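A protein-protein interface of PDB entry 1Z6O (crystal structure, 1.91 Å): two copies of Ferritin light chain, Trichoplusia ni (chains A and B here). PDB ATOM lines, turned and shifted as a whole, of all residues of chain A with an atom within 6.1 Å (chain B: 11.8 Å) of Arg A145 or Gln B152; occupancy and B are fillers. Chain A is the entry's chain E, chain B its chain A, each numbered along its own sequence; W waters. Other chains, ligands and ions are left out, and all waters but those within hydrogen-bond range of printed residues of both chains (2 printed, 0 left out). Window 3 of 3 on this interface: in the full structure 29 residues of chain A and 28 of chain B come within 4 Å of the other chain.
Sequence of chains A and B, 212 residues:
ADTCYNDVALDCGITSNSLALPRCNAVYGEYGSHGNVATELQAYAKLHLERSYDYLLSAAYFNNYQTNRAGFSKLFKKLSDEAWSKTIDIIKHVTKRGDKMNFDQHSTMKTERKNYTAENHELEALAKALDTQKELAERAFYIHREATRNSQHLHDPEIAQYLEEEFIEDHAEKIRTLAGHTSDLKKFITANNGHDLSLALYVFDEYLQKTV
The backbone carbonyl oxygen (O) of Ser B151 lies within hydrogen-bond range of the guanidinium group (NH2) of Arg A149. The backbone carbonyl oxygen (O) of Gln B152 sits at hydrogen-bond distance from the guanidinium group (NH2) of Arg A145 (2.5 Å). O of Leu B154 is in hydrogen-bond range of NH1 of Arg A149 (2.8 Å). NE2 of His B155 lies within hydrogen-bond range of ND1 of His A144 (2.8 Å). A ring nitrogen (ND1) of His B155 is in hydrogen-bond range of the guanidinium group (NH1) of Arg A149 (3.2 Å).
Among the printed residues, pairs that only touch across the chains: Phe A141 with His B155, Phe A141 with Asp B156, Phe A141 with Pro B157, Phe A141 with Glu B158, His A144 with Pro B157, Arg A145 with His B155, Arg A149 with Thr B148, Arg A149 with Arg B149 and Arg A149 with Gln B152.
OG1 of Thr B148 lies within hydrogen-bond range of O of His B144 (2.9 Å). The backbone carbonyl oxygen of Ala B147 sits at hydrogen-bond distance from the backbone NH of Asp B156 (2.8 Å). The backbone NH of Glu B158 sits close to the side-chain carboxylate of Asp B156, 3.2 Å away. The side-chain hydroxyl (OG1) of Thr A148 is in hydrogen-bond range of the backbone carbonyl oxygen (O) of His A144. The backbone carbonyl oxygen of Arg A145 sits at hydrogen-bond distance from the backbone NH of Asn A150.
Arg A149 touches Thr B148, but with the chains exchanged Thr A148 does not touch Arg B149 (7.7 Å). Arg A149 touches its own counterpart, Arg B149. Arg A149 touches Ser B151, but with the chains exchanged Ser A151 does not touch Arg B149 (12.2 Å). 8 positions are printed for both chains.
Arg A145 touches just these residues of chain B: Gln B152 (2.5 Å) and His B155 (3.5 Å). Gln B152 touches just these residues of chain A: Arg A145 and Arg A149. Of chain B, only His B155 and Pro B157 come within 4 Å of His A144. No residue of chain B comes within 4 Å of Ala A147. Thr A148 touches none of the printed residues of chain B. Asn A150 touches none of the printed residues of chain B. Printed residues of chain A within 4 Å of Leu B154: Arg A149 (2.8 Å). Printed residues of chain A within 4 Å of Arg B149: Arg A149 (3.6 Å). Of the printed residues of chain A, Glu B158 touches Phe A141 (3.9 Å). Of the printed residues of chain A, Pro B157 touches Phe A141 and His A144. Printed residues of chain B within 4 Å of Phe A141: His B155 (3.5 Å), Asp B156 (3.7 Å), Pro B157 (3.5 Å) and Glu B158 (3.9 Å). Glu B30 touches none of the printed residues of chain A. The nearest residue of chain A that does not touch Gln B152 is Asn A150 (5.3 Å).
Hydrophobic or aromatic side chains of chain A that line the printed part of chain B: Phe A141 and His A144. Along chain A the printed residues that touch a printed residue of chain B span positions 141 to 149. Of the 24 printed residues of chain B, 9 touch a printed residue of chain A. Among the printed residues, 14 pairs touch across the chains. Among the printed residues, no Asp or Glu carboxylate lies within 4 Å of a Lys or Arg side-chain nitrogen of the other chain.
Water W1 lies within hydrogen-bond range of OD1 of Asn A150 (2.9 Å), NH2 of Arg A145 (3.1 Å) and NE2 of Gln B152 (3.5 Å). Water W2 lies within hydrogen-bond range of the backbone carbonyl oxygen (O) of Arg B149 and the guanidinium group (NE) of Arg A149.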
ATOM      1  N   ALA A 140      -4.985  -5.490  -3.782  1.00  0.00           N
ATOM      2  CA  ALA A 140      -5.598  -5.880  -2.511  1.00  0.00           C
ATOM      3  C   ALA A 140      -4.563  -6.607  -1.643  1.00  0.00           C
ATOM      4  O   ALA A 140      -4.528  -6.412  -0.433  1.00  0.00           O
ATOM      5  CB  ALA A 140      -6.827  -6.788  -2.741  1.00  0.00           C
ATOM      6  N   PHE A 141      -3.733  -7.452  -2.254  1.00  0.00           N
ATOM      7  CA  PHE A 141      -2.695  -8.172  -1.497  1.00  0.00           C
ATOM      8  C   PHE A 141      -1.739  -7.159  -0.855  1.00  0.00           C
ATOM      9  O   PHE A 141      -1.303  -7.320   0.280  1.00  0.00           O
ATOM     10  CB  PHE A 141      -1.871  -9.078  -2.426  1.00  0.00           C
ATOM     11  CG  PHE A 141      -2.506 -10.425  -2.721  1.00  0.00           C
ATOM     12  CD1 PHE A 141      -3.862 -10.659  -2.476  1.00  0.00           C
ATOM     13  CD2 PHE A 141      -1.730 -11.456  -3.257  1.00  0.00           C
ATOM     14  CE1 PHE A 141      -4.443 -11.915  -2.764  1.00  0.00           C
ATOM     15  CE2 PHE A 141      -2.295 -12.710  -3.549  1.00  0.00           C
ATOM     16  CZ  PHE A 141      -3.661 -12.936  -3.301  1.00  0.00           C
ATOM     17  N   TYR A 142      -1.405  -6.124  -1.611  1.00  0.00           N
ATOM     18  CA  TYR A 142      -0.493  -5.080  -1.139  1.00  0.00           C
ATOM     19  C   TYR A 142      -1.071  -4.319   0.066  1.00  0.00           C
ATOM     20  O   TYR A 142      -0.395  -4.116   1.071  1.00  0.00           O
ATOM     21  CB  TYR A 142      -0.219  -4.112  -2.291  1.00  0.00           C
ATOM     22  CG  TYR A 142       0.697  -2.975  -1.925  1.00  0.00           C
ATOM     23  CD1 TYR A 142       2.066  -3.180  -1.781  1.00  0.00           C
ATOM     24  CD2 TYR A 142       0.193  -1.693  -1.719  1.00  0.00           C
ATOM     25  CE1 TYR A 142       2.917  -2.132  -1.438  1.00  0.00           C
ATOM     26  CE2 TYR A 142       1.033  -0.635  -1.374  1.00  0.00           C
ATOM     27  CZ  TYR A 142       2.395  -0.865  -1.236  1.00  0.00           C
ATOM     28  OH  TYR A 142       3.235   0.172  -0.904  1.00  0.00           O
ATOM     29  N   ILE A 143      -2.324  -3.892  -0.031  1.00  0.00           N
ATOM     30  CA  ILE A 143      -2.944  -3.163   1.077  1.00  0.00           C
ATOM     31  C   ILE A 143      -3.062  -4.065   2.306  1.00  0.00           C
ATOM     32  O   ILE A 143      -2.852  -3.631   3.447  1.00  0.00           O
ATOM     33  CB  ILE A 143      -4.339  -2.644   0.667  1.00  0.00           C
ATOM     34  CG1 ILE A 143      -4.192  -1.703  -0.534  1.00  0.00           C
ATOM     35  CG2 ILE A 143      -5.003  -1.892   1.833  1.00  0.00           C
ATOM     36  CD1 ILE A 143      -5.543  -1.284  -1.135  1.00  0.00           C
ATOM     37  N   HIS A 144      -3.391  -5.331   2.067  1.00  0.00           N
ATOM     38  CA  HIS A 144      -3.525  -6.309   3.144  1.00  0.00           C
ATOM     39  C   HIS A 144      -2.178  -6.451   3.876  1.00  0.00           C
ATOM     40  O   HIS A 144      -2.118  -6.466   5.108  1.00  0.00           O
ATOM     41  CB  HIS A 144      -3.965  -7.651   2.539  1.00  0.00           C
ATOM     42  CG  HIS A 144      -4.284  -8.708   3.550  1.00  0.00           C
ATOM     43  ND1 HIS A 144      -3.312  -9.398   4.242  1.00  0.00           N
ATOM     44  CD2 HIS A 144      -5.476  -9.219   3.958  1.00  0.00           C
ATOM     45  CE1 HIS A 144      -3.888 -10.292   5.032  1.00  0.00           C
ATOM     46  NE2 HIS A 144      -5.200 -10.203   4.876  1.00  0.00           N
ATOM     47  N   ARG A 145      -1.096  -6.549   3.112  1.00  0.00           N
ATOM     48  CA  ARG A 145       0.241  -6.677   3.698  1.00  0.00           C
ATOM     49  C   ARG A 145       0.629  -5.392   4.461  1.00  0.00           C
ATOM     50  O   ARG A 145       1.262  -5.436   5.525  1.00  0.00           O
ATOM     51  CB  ARG A 145       1.268  -6.955   2.588  1.00  0.00           C
ATOM     52  CG  ARG A 145       2.634  -7.304   3.137  1.00  0.00           C
ATOM     53  CD  ARG A 145       3.657  -7.669   2.060  1.00  0.00           C
ATOM     54  NE  ARG A 145       4.907  -7.994   2.736  1.00  0.00           N
ATOM     55  CZ  ARG A 145       5.766  -8.921   2.343  1.00  0.00           C
ATOM     56  NH1 ARG A 145       5.531  -9.642   1.249  1.00  0.00           N
ATOM     57  NH2 ARG A 145       6.851  -9.143   3.073  1.00  0.00           N
ATOM     58  N   GLU A 146       0.247  -4.249   3.912  1.00  0.00           N
ATOM     59  CA  GLU A 146       0.533  -2.973   4.562  1.00  0.00           C
ATOM     60  C   GLU A 146      -0.225  -2.889   5.895  1.00  0.00           C
ATOM     61  O   GLU A 146       0.264  -2.319   6.866  1.00  0.00           O
ATOM     62  CB  GLU A 146       0.106  -1.835   3.627  1.00  0.00           C
ATOM     63  CG  GLU A 146       0.416  -0.440   4.115  1.00  0.00           C
ATOM     64  CD  GLU A 146       1.911  -0.175   4.258  1.00  0.00           C
ATOM     65  OE1 GLU A 146       2.712  -0.756   3.476  1.00  0.00           O
ATOM     66  OE2 GLU A 146       2.269   0.628   5.149  1.00  0.00           O
ATOM     67  N   ALA A 147      -1.418  -3.474   5.952  1.00  0.00           N
ATOM     68  CA  ALA A 147      -2.222  -3.430   7.167  1.00  0.00           C
ATOM     69  C   ALA A 147      -1.802  -4.387   8.276  1.00  0.00           C
ATOM     70  O   ALA A 147      -2.073  -4.140   9.447  1.00  0.00           O
ATOM     71  CB  ALA A 147      -3.700  -3.718   6.820  1.00  0.00           C
ATOM     72  N   THR A 148      -1.133  -5.476   7.922  1.00  0.00           N
ATOM     73  CA  THR A 148      -0.849  -6.485   8.929  1.00  0.00           C
ATOM     74  C   THR A 148       0.568  -7.007   8.970  1.00  0.00           C
ATOM     75  O   THR A 148       0.842  -7.950   9.696  1.00  0.00           O
ATOM     76  CB  THR A 148      -1.755  -7.729   8.686  1.00  0.00           C
ATOM     77  OG1 THR A 148      -1.501  -8.244   7.367  1.00  0.00           O
ATOM     78  CG2 THR A 148      -3.220  -7.363   8.790  1.00  0.00           C
ATOM     79  N   ARG A 149       1.474  -6.401   8.229  1.00  0.00           N
ATOM     80  CA  ARG A 149       2.801  -6.967   8.198  1.00  0.00           C
ATOM     81  C   ARG A 149       3.956  -6.013   7.930  1.00  0.00           C
ATOM     82  O   ARG A 149       5.017  -6.154   8.520  1.00  0.00           O
ATOM     83  CB  ARG A 149       2.769  -8.070   7.136  1.00  0.00           C
ATOM     84  CG  ARG A 149       3.920  -8.992   7.092  1.00  0.00           C
ATOM     85  CD  ARG A 149       3.618 -10.138   6.121  1.00  0.00           C
ATOM     86  NE  ARG A 149       4.826 -10.914   5.935  1.00  0.00           N
ATOM     87  CZ  ARG A 149       5.006 -11.825   4.997  1.00  0.00           C
ATOM     88  NH1 ARG A 149       4.034 -12.096   4.124  1.00  0.00           N
ATOM     89  NH2 ARG A 149       6.169 -12.455   4.935  1.00  0.00           N
ATOM     90  N   ASN A 150       3.754  -5.034   7.061  1.00  0.00           N
ATOM     91  CA  ASN A 150       4.857  -4.153   6.695  1.00  0.00           C
ATOM     92  C   ASN A 150       5.338  -3.122   7.684  1.00  0.00           C
ATOM     93  O   ASN A 150       6.506  -2.763   7.663  1.00  0.00           O
ATOM     94  CB  ASN A 150       4.557  -3.436   5.383  1.00  0.00           C
ATOM     95  CG  ASN A 150       4.579  -4.372   4.196  1.00  0.00           C
ATOM     96  OD1 ASN A 150       5.138  -5.474   4.265  1.00  0.00           O
ATOM     97  ND2 ASN A 150       3.981  -3.934   3.093  1.00  0.00           N
ATOM     98  N   SER A 151       4.452  -2.631   8.537  1.00  0.00           N
ATOM     99  CA  SER A 151       4.840  -1.599   9.489  1.00  0.00           C
ATOM    100  C   SER A 151       4.698  -2.084  10.918  1.00  0.00           C
ATOM    101  O   SER A 151       3.631  -2.540  11.338  1.00  0.00           O
ATOM    102  CB  SER A 151       3.997  -0.340   9.255  1.00  0.00           C
ATOM    103  OG  SER A 151       4.322   0.673  10.190  1.00  0.00           O
ATOM    104  N   GLY B  29      -0.090 -12.722  -7.729  1.00  0.00           N
ATOM    105  CA  GLY B  29       0.542 -12.667  -6.419  1.00  0.00           C
ATOM    106  C   GLY B  29       1.741 -13.617  -6.402  1.00  0.00           C
ATOM    107  O   GLY B  29       2.164 -14.089  -5.352  1.00  0.00           O
ATOM    108  N   GLU B  30       2.299 -13.910  -7.567  1.00  0.00           N
ATOM    109  CA  GLU B  30       3.429 -14.858  -7.645  1.00  0.00           C
ATOM    110  C   GLU B  30       3.153 -16.210  -6.956  1.00  0.00           C
ATOM    111  O   GLU B  30       4.052 -16.838  -6.367  1.00  0.00           O
ATOM    112  CB  GLU B  30       4.687 -14.225  -7.049  1.00  0.00           C
ATOM    113  CG  GLU B  30       5.180 -13.025  -7.846  1.00  0.00           C
ATOM    114  CD  GLU B  30       6.425 -12.407  -7.254  1.00  0.00           C
ATOM    115  OE1 GLU B  30       6.383 -12.013  -6.068  1.00  0.00           O
ATOM    116  OE2 GLU B  30       7.444 -12.317  -7.974  1.00  0.00           O
ATOM    117  N   TYR B  31       1.904 -16.656  -7.029  1.00  0.00           N
ATOM    118  CA  TYR B  31       1.511 -17.927  -6.427  1.00  0.00           C
ATOM    119  C   TYR B  31       2.377 -19.036  -7.016  1.00  0.00           C
ATOM    120  O   TYR B  31       2.461 -19.181  -8.234  1.00  0.00           O
ATOM    121  CB  TYR B  31       0.044 -18.223  -6.750  1.00  0.00           C
ATOM    122  CG  TYR B  31      -0.472 -19.487  -6.119  1.00  0.00           C
ATOM    123  CD1 TYR B  31      -0.849 -19.509  -4.781  1.00  0.00           C
ATOM    124  CD2 TYR B  31      -0.575 -20.662  -6.856  1.00  0.00           C
ATOM    125  CE1 TYR B  31      -1.320 -20.669  -4.188  1.00  0.00           C
ATOM    126  CE2 TYR B  31      -1.047 -21.839  -6.270  1.00  0.00           C
ATOM    127  CZ  TYR B  31      -1.415 -21.827  -4.932  1.00  0.00           C
ATOM    128  OH  TYR B  31      -1.863 -22.977  -4.337  1.00  0.00           O
ATOM    129  N   SER B  33       5.593 -19.222  -7.026  1.00  0.00           N
ATOM    130  CA  SER B  33       6.956 -18.752  -7.322  1.00  0.00           C
ATOM    131  C   SER B  33       7.862 -18.626  -6.104  1.00  0.00           C
ATOM    132  O   SER B  33       9.047 -18.938  -6.173  1.00  0.00           O
ATOM    133  CB  SER B  33       6.913 -17.395  -8.032  1.00  0.00           C
ATOM    134  OG  SER B  33       6.216 -17.494  -9.258  1.00  0.00           O
ATOM    135  N   HIS B  34       7.314 -18.146  -4.996  1.00  0.00           N
ATOM    136  CA  HIS B  34       8.096 -17.989  -3.775  1.00  0.00           C
ATOM    137  C   HIS B  34       7.453 -18.841  -2.696  1.00  0.00           C
ATOM    138  O   HIS B  34       6.240 -19.042  -2.706  1.00  0.00           O
ATOM    139  CB  HIS B  34       8.092 -16.525  -3.310  1.00  0.00           C
ATOM    140  CG  HIS B  34       8.688 -15.571  -4.295  1.00  0.00           C
ATOM    141  ND1 HIS B  34      10.049 -15.447  -4.484  1.00  0.00           N
ATOM    142  CD2 HIS B  34       8.109 -14.700  -5.155  1.00  0.00           C
ATOM    143  CE1 HIS B  34      10.281 -14.542  -5.416  1.00  0.00           C
ATOM    144  NE2 HIS B  34       9.121 -14.072  -5.841  1.00  0.00           N
ATOM    145  N   GLY B  35       8.264 -19.342  -1.771  1.00  0.00           N
ATOM    146  CA  GLY B  35       7.732 -20.141  -0.683  1.00  0.00           C
ATOM    147  C   GLY B  35       7.210 -21.521  -1.036  1.00  0.00           C
ATOM    148  O   GLY B  35       7.333 -21.994  -2.165  1.00  0.00           O
ATOM    149  N   ASN B  36       6.593 -22.159  -0.051  1.00  0.00           N
ATOM    150  CA  ASN B  36       6.077 -23.505  -0.212  1.00  0.00           C
ATOM    151  C   ASN B  36       4.561 -23.591  -0.158  1.00  0.00           C
ATOM    152  O   ASN B  36       4.023 -24.690  -0.065  1.00  0.00           O
ATOM    153  CB  ASN B  36       6.630 -24.394   0.899  1.00  0.00           C
ATOM    154  CG  ASN B  36       8.140 -24.439   0.909  1.00  0.00           C
ATOM    155  OD1 ASN B  36       8.768 -24.677  -0.119  1.00  0.00           O
ATOM    156  ND2 ASN B  36       8.732 -24.216   2.078  1.00  0.00           N
ATOM    157  N   VAL B  37       3.869 -22.460  -0.217  1.00  0.00           N
ATOM    158  CA  VAL B  37       2.422 -22.525  -0.098  1.00  0.00           C
ATOM    159  C   VAL B  37       1.754 -23.378  -1.169  1.00  0.00           C
ATOM    160  O   VAL B  37       0.893 -24.191  -0.851  1.00  0.00           O
ATOM    161  CB  VAL B  37       1.771 -21.115  -0.076  1.00  0.00           C
ATOM    162  CG1 VAL B  37       1.934 -20.426  -1.407  1.00  0.00           C
ATOM    163  CG2 VAL B  37       0.286 -21.242   0.243  1.00  0.00           C
ATOM    164  N   HIS B 144      -1.081 -21.728   6.548  1.00  0.00           N
ATOM    165  CA  HIS B 144      -1.526 -20.355   6.775  1.00  0.00           C
ATOM    166  C   HIS B 144      -0.310 -19.475   7.122  1.00  0.00           C
ATOM    167  O   HIS B 144      -0.154 -18.367   6.604  1.00  0.00           O
ATOM    168  CB  HIS B 144      -2.549 -20.353   7.921  1.00  0.00           C
ATOM    169  CG  HIS B 144      -3.201 -19.027   8.164  1.00  0.00           C
ATOM    170  ND1 HIS B 144      -2.560 -17.985   8.803  1.00  0.00           N
ATOM    171  CD2 HIS B 144      -4.454 -18.586   7.883  1.00  0.00           C
ATOM    172  CE1 HIS B 144      -3.392 -16.960   8.910  1.00  0.00           C
ATOM    173  NE2 HIS B 144      -4.547 -17.300   8.360  1.00  0.00           N
ATOM    174  N   ARG B 145       0.554 -19.976   7.998  1.00  0.00           N
ATOM    175  CA  ARG B 145       1.753 -19.233   8.395  1.00  0.00           C
ATOM    176  C   ARG B 145       2.719 -19.076   7.202  1.00  0.00           C
ATOM    177  O   ARG B 145       3.364 -18.034   7.022  1.00  0.00           O
ATOM    178  CB  ARG B 145       2.459 -19.970   9.546  1.00  0.00           C
ATOM    179  CG  ARG B 145       3.587 -19.159  10.146  1.00  0.00           C
ATOM    180  CD  ARG B 145       4.255 -19.827  11.348  1.00  0.00           C
ATOM    181  NE  ARG B 145       5.300 -18.928  11.825  1.00  0.00           N
ATOM    182  CZ  ARG B 145       5.641 -18.761  13.092  1.00  0.00           C
ATOM    183  NH1 ARG B 145       5.024 -19.442  14.054  1.00  0.00           N
ATOM    184  NH2 ARG B 145       6.586 -17.879  13.393  1.00  0.00           N
ATOM    185  N   GLU B 146       2.817 -20.117   6.389  1.00  0.00           N
ATOM    186  CA  GLU B 146       3.678 -20.070   5.211  1.00  0.00           C
ATOM    187  C   GLU B 146       3.150 -19.016   4.225  1.00  0.00           C
ATOM    188  O   GLU B 146       3.920 -18.346   3.543  1.00  0.00           O
ATOM    189  CB  GLU B 146       3.699 -21.456   4.557  1.00  0.00           C
ATOM    190  CG  GLU B 146       4.618 -21.602   3.367  1.00  0.00           C
ATOM    191  CD  GLU B 146       6.089 -21.407   3.721  1.00  0.00           C
ATOM    192  OE1 GLU B 146       6.492 -21.745   4.868  1.00  0.00           O
ATOM    193  OE2 GLU B 146       6.833 -20.926   2.836  1.00  0.00           O
ATOM    194  N   ALA B 147       1.830 -18.855   4.160  1.00  0.00           N
ATOM    195  CA  ALA B 147       1.234 -17.894   3.240  1.00  0.00           C
ATOM    196  C   ALA B 147       1.300 -16.434   3.671  1.00  0.00           C
ATOM    197  O   ALA B 147       1.265 -15.537   2.834  1.00  0.00           O
ATOM    198  CB  ALA B 147      -0.248 -18.257   3.003  1.00  0.00           C
ATOM    199  N   THR B 148       1.404 -16.184   4.968  1.00  0.00           N
ATOM    200  CA  THR B 148       1.315 -14.808   5.429  1.00  0.00           C
ATOM    201  C   THR B 148       2.369 -14.365   6.415  1.00  0.00           C
ATOM    202  O   THR B 148       2.276 -13.268   6.946  1.00  0.00           O
ATOM    203  CB  THR B 148      -0.053 -14.584   6.138  1.00  0.00           C
ATOM    204  OG1 THR B 148      -0.161 -15.497   7.244  1.00  0.00           O
ATOM    205  CG2 THR B 148      -1.206 -14.836   5.188  1.00  0.00           C
ATOM    206  N   ARG B 149       3.379 -15.179   6.652  1.00  0.00           N
ATOM    207  CA  ARG B 149       4.327 -14.791   7.668  1.00  0.00           C
ATOM    208  C   ARG B 149       5.751 -15.309   7.522  1.00  0.00           C
ATOM    209  O   ARG B 149       6.697 -14.591   7.812  1.00  0.00           O
ATOM    210  CB  ARG B 149       3.732 -15.252   9.003  1.00  0.00           C
ATOM    211  CG  ARG B 149       4.369 -14.740  10.232  1.00  0.00           C
ATOM    212  CD  ARG B 149       3.520 -15.132  11.447  1.00  0.00           C
ATOM    213  NE  ARG B 149       4.258 -14.804  12.648  1.00  0.00           N
ATOM    214  CZ  ARG B 149       3.947 -15.213  13.864  1.00  0.00           C
ATOM    215  NH1 ARG B 149       2.879 -15.988  14.064  1.00  0.00           N
ATOM    216  NH2 ARG B 149       4.717 -14.845  14.876  1.00  0.00           N
ATOM    217  N   ASN B 150       5.912 -16.539   7.059  1.00  0.00           N
ATOM    218  CA  ASN B 150       7.249 -17.117   6.992  1.00  0.00           C
ATOM    219  C   ASN B 150       8.211 -16.636   5.935  1.00  0.00           C
ATOM    220  O   ASN B 150       9.412 -16.668   6.152  1.00  0.00           O
ATOM    221  CB  ASN B 150       7.171 -18.637   6.892  1.00  0.00           C
ATOM    222  CG  ASN B 150       6.685 -19.275   8.174  1.00  0.00           C
ATOM    223  OD1 ASN B 150       6.722 -18.657   9.246  1.00  0.00           O
ATOM    224  ND2 ASN B 150       6.238 -20.522   8.077  1.00  0.00           N
ATOM    225  N   SER B 151       7.699 -16.205   4.791  1.00  0.00           N
ATOM    226  CA  SER B 151       8.574 -15.768   3.713  1.00  0.00           C
ATOM    227  C   SER B 151       8.364 -14.302   3.391  1.00  0.00           C
ATOM    228  O   SER B 151       7.247 -13.859   3.113  1.00  0.00           O
ATOM    229  CB  SER B 151       8.334 -16.637   2.473  1.00  0.00           C
ATOM    230  OG  SER B 151       9.144 -16.216   1.389  1.00  0.00           O
ATOM    231  N   GLN B 152       9.454 -13.549   3.443  1.00  0.00           N
ATOM    232  CA  GLN B 152       9.428 -12.120   3.172  1.00  0.00           C
ATOM    233  C   GLN B 152       8.811 -11.769   1.823  1.00  0.00           C
ATOM    234  O   GLN B 152       8.139 -10.753   1.693  1.00  0.00           O
ATOM    235  CB  GLN B 152      10.857 -11.570   3.228  1.00  0.00           C
ATOM    236  CG  GLN B 152      10.989 -10.082   2.940  1.00  0.00           C
ATOM    237  CD  GLN B 152      10.190  -9.218   3.898  1.00  0.00           C
ATOM    238  OE1 GLN B 152      10.053  -9.541   5.080  1.00  0.00           O
ATOM    239  NE2 GLN B 152       9.671  -8.102   3.394  1.00  0.00           N
ATOM    240  N   HIS B 153       9.026 -12.609   0.818  1.00  0.00           N
ATOM    241  CA  HIS B 153       8.514 -12.299  -0.512  1.00  0.00           C
ATOM    242  C   HIS B 153       7.185 -12.937  -0.873  1.00  0.00           C
ATOM    243  O   HIS B 153       6.714 -12.813  -2.001  1.00  0.00           O
ATOM    244  CB  HIS B 153       9.569 -12.668  -1.550  1.00  0.00           C
ATOM    245  CG  HIS B 153      10.898 -12.040  -1.279  1.00  0.00           C
ATOM    246  ND1 HIS B 153      11.077 -10.673  -1.236  1.00  0.00           N
ATOM    247  CD2 HIS B 153      12.095 -12.586  -0.958  1.00  0.00           C
ATOM    248  CE1 HIS B 153      12.325 -10.405  -0.898  1.00  0.00           C
ATOM    249  NE2 HIS B 153      12.963 -11.547  -0.723  1.00  0.00           N
ATOM    250  N   LEU B 154       6.575 -13.622   0.078  1.00  0.00           N
ATOM    251  CA  LEU B 154       5.293 -14.249  -0.201  1.00  0.00           C
ATOM    252  C   LEU B 154       4.231 -13.756   0.772  1.00  0.00           C
ATOM    253  O   LEU B 154       4.406 -13.836   1.987  1.00  0.00           O
ATOM    254  CB  LEU B 154       5.423 -15.776  -0.095  1.00  0.00           C
ATOM    255  CG  LEU B 154       4.135 -16.619  -0.049  1.00  0.00           C
ATOM    256  CD1 LEU B 154       3.323 -16.410  -1.305  1.00  0.00           C
ATOM    257  CD2 LEU B 154       4.505 -18.090   0.100  1.00  0.00           C
ATOM    258  N   HIS B 155       3.148 -13.207   0.233  1.00  0.00           N
ATOM    259  CA  HIS B 155       2.026 -12.790   1.064  1.00  0.00           C
ATOM    260  C   HIS B 155       0.793 -13.172   0.257  1.00  0.00           C
ATOM    261  O   HIS B 155       0.480 -12.530  -0.749  1.00  0.00           O
ATOM    262  CB  HIS B 155       2.018 -11.285   1.339  1.00  0.00           C
ATOM    263  CG  HIS B 155       0.976 -10.880   2.337  1.00  0.00           C
ATOM    264  ND1 HIS B 155       1.011 -11.296   3.653  1.00  0.00           N
ATOM    265  CD2 HIS B 155      -0.162 -10.154   2.202  1.00  0.00           C
ATOM    266  CE1 HIS B 155      -0.060 -10.844   4.285  1.00  0.00           C
ATOM    267  NE2 HIS B 155      -0.790 -10.149   3.428  1.00  0.00           N
ATOM    268  N   ASP B 156       0.108 -14.235   0.673  1.00  0.00           N
ATOM    269  CA  ASP B 156      -1.078 -14.668  -0.062  1.00  0.00           C
ATOM    270  C   ASP B 156      -2.283 -14.794   0.863  1.00  0.00           C
ATOM    271  O   ASP B 156      -2.567 -15.859   1.415  1.00  0.00           O
ATOM    272  CB  ASP B 156      -0.821 -15.994  -0.775  1.00  0.00           C
ATOM    273  CG  ASP B 156      -1.794 -16.214  -1.916  1.00  0.00           C
ATOM    274  OD1 ASP B 156      -3.018 -16.194  -1.652  1.00  0.00           O
ATOM    275  OD2 ASP B 156      -1.348 -16.375  -3.073  1.00  0.00           O
ATOM    276  N   PRO B 157      -3.002 -13.687   1.050  1.00  0.00           N
ATOM    277  CA  PRO B 157      -4.174 -13.706   1.925  1.00  0.00           C
ATOM    278  C   PRO B 157      -5.365 -14.449   1.330  1.00  0.00           C
ATOM    279  O   PRO B 157      -6.332 -14.720   2.039  1.00  0.00           O
ATOM    280  CB  PRO B 157      -4.450 -12.220   2.179  1.00  0.00           C
ATOM    281  CG  PRO B 157      -3.961 -11.557   0.923  1.00  0.00           C
ATOM    282  CD  PRO B 157      -2.695 -12.322   0.571  1.00  0.00           C
ATOM    283  N   GLU B 158      -5.303 -14.781   0.041  1.00  0.00           N
ATOM    284  CA  GLU B 158      -6.402 -15.533  -0.570  1.00  0.00           C
ATOM    285  C   GLU B 158      -6.334 -16.952  -0.001  1.00  0.00           C
ATOM    286  O   GLU B 158      -7.351 -17.516   0.409  1.00  0.00           O
ATOM    287  CB  GLU B 158      -6.275 -15.558  -2.099  1.00  0.00           C
ATOM    288  CG  GLU B 158      -7.551 -16.046  -2.818  1.00  0.00           C
ATOM    289  CD  GLU B 158      -7.764 -17.566  -2.767  1.00  0.00           C
ATOM    290  OE1 GLU B 158      -8.944 -17.989  -2.696  1.00  0.00           O
ATOM    291  OE2 GLU B 158      -6.776 -18.340  -2.818  1.00  0.00           O
ATOM    292  N   ALA B 160      -4.842 -17.742   2.789  1.00  0.00           N
ATOM    293  CA  ALA B 160      -5.120 -17.613   4.221  1.00  0.00           C
ATOM    294  C   ALA B 160      -6.627 -17.586   4.519  1.00  0.00           C
ATOM    295  O   ALA B 160      -7.104 -18.300   5.404  1.00  0.00           O
ATOM    296  CB  ALA B 160      -4.450 -16.347   4.779  1.00  0.00           C
HETATM  297  O   HOH W   1       7.004  -7.305   5.513  1.00  0.00           O
HETATM  298  O   HOH W   2       6.513 -11.649   8.709  1.00  0.00           O
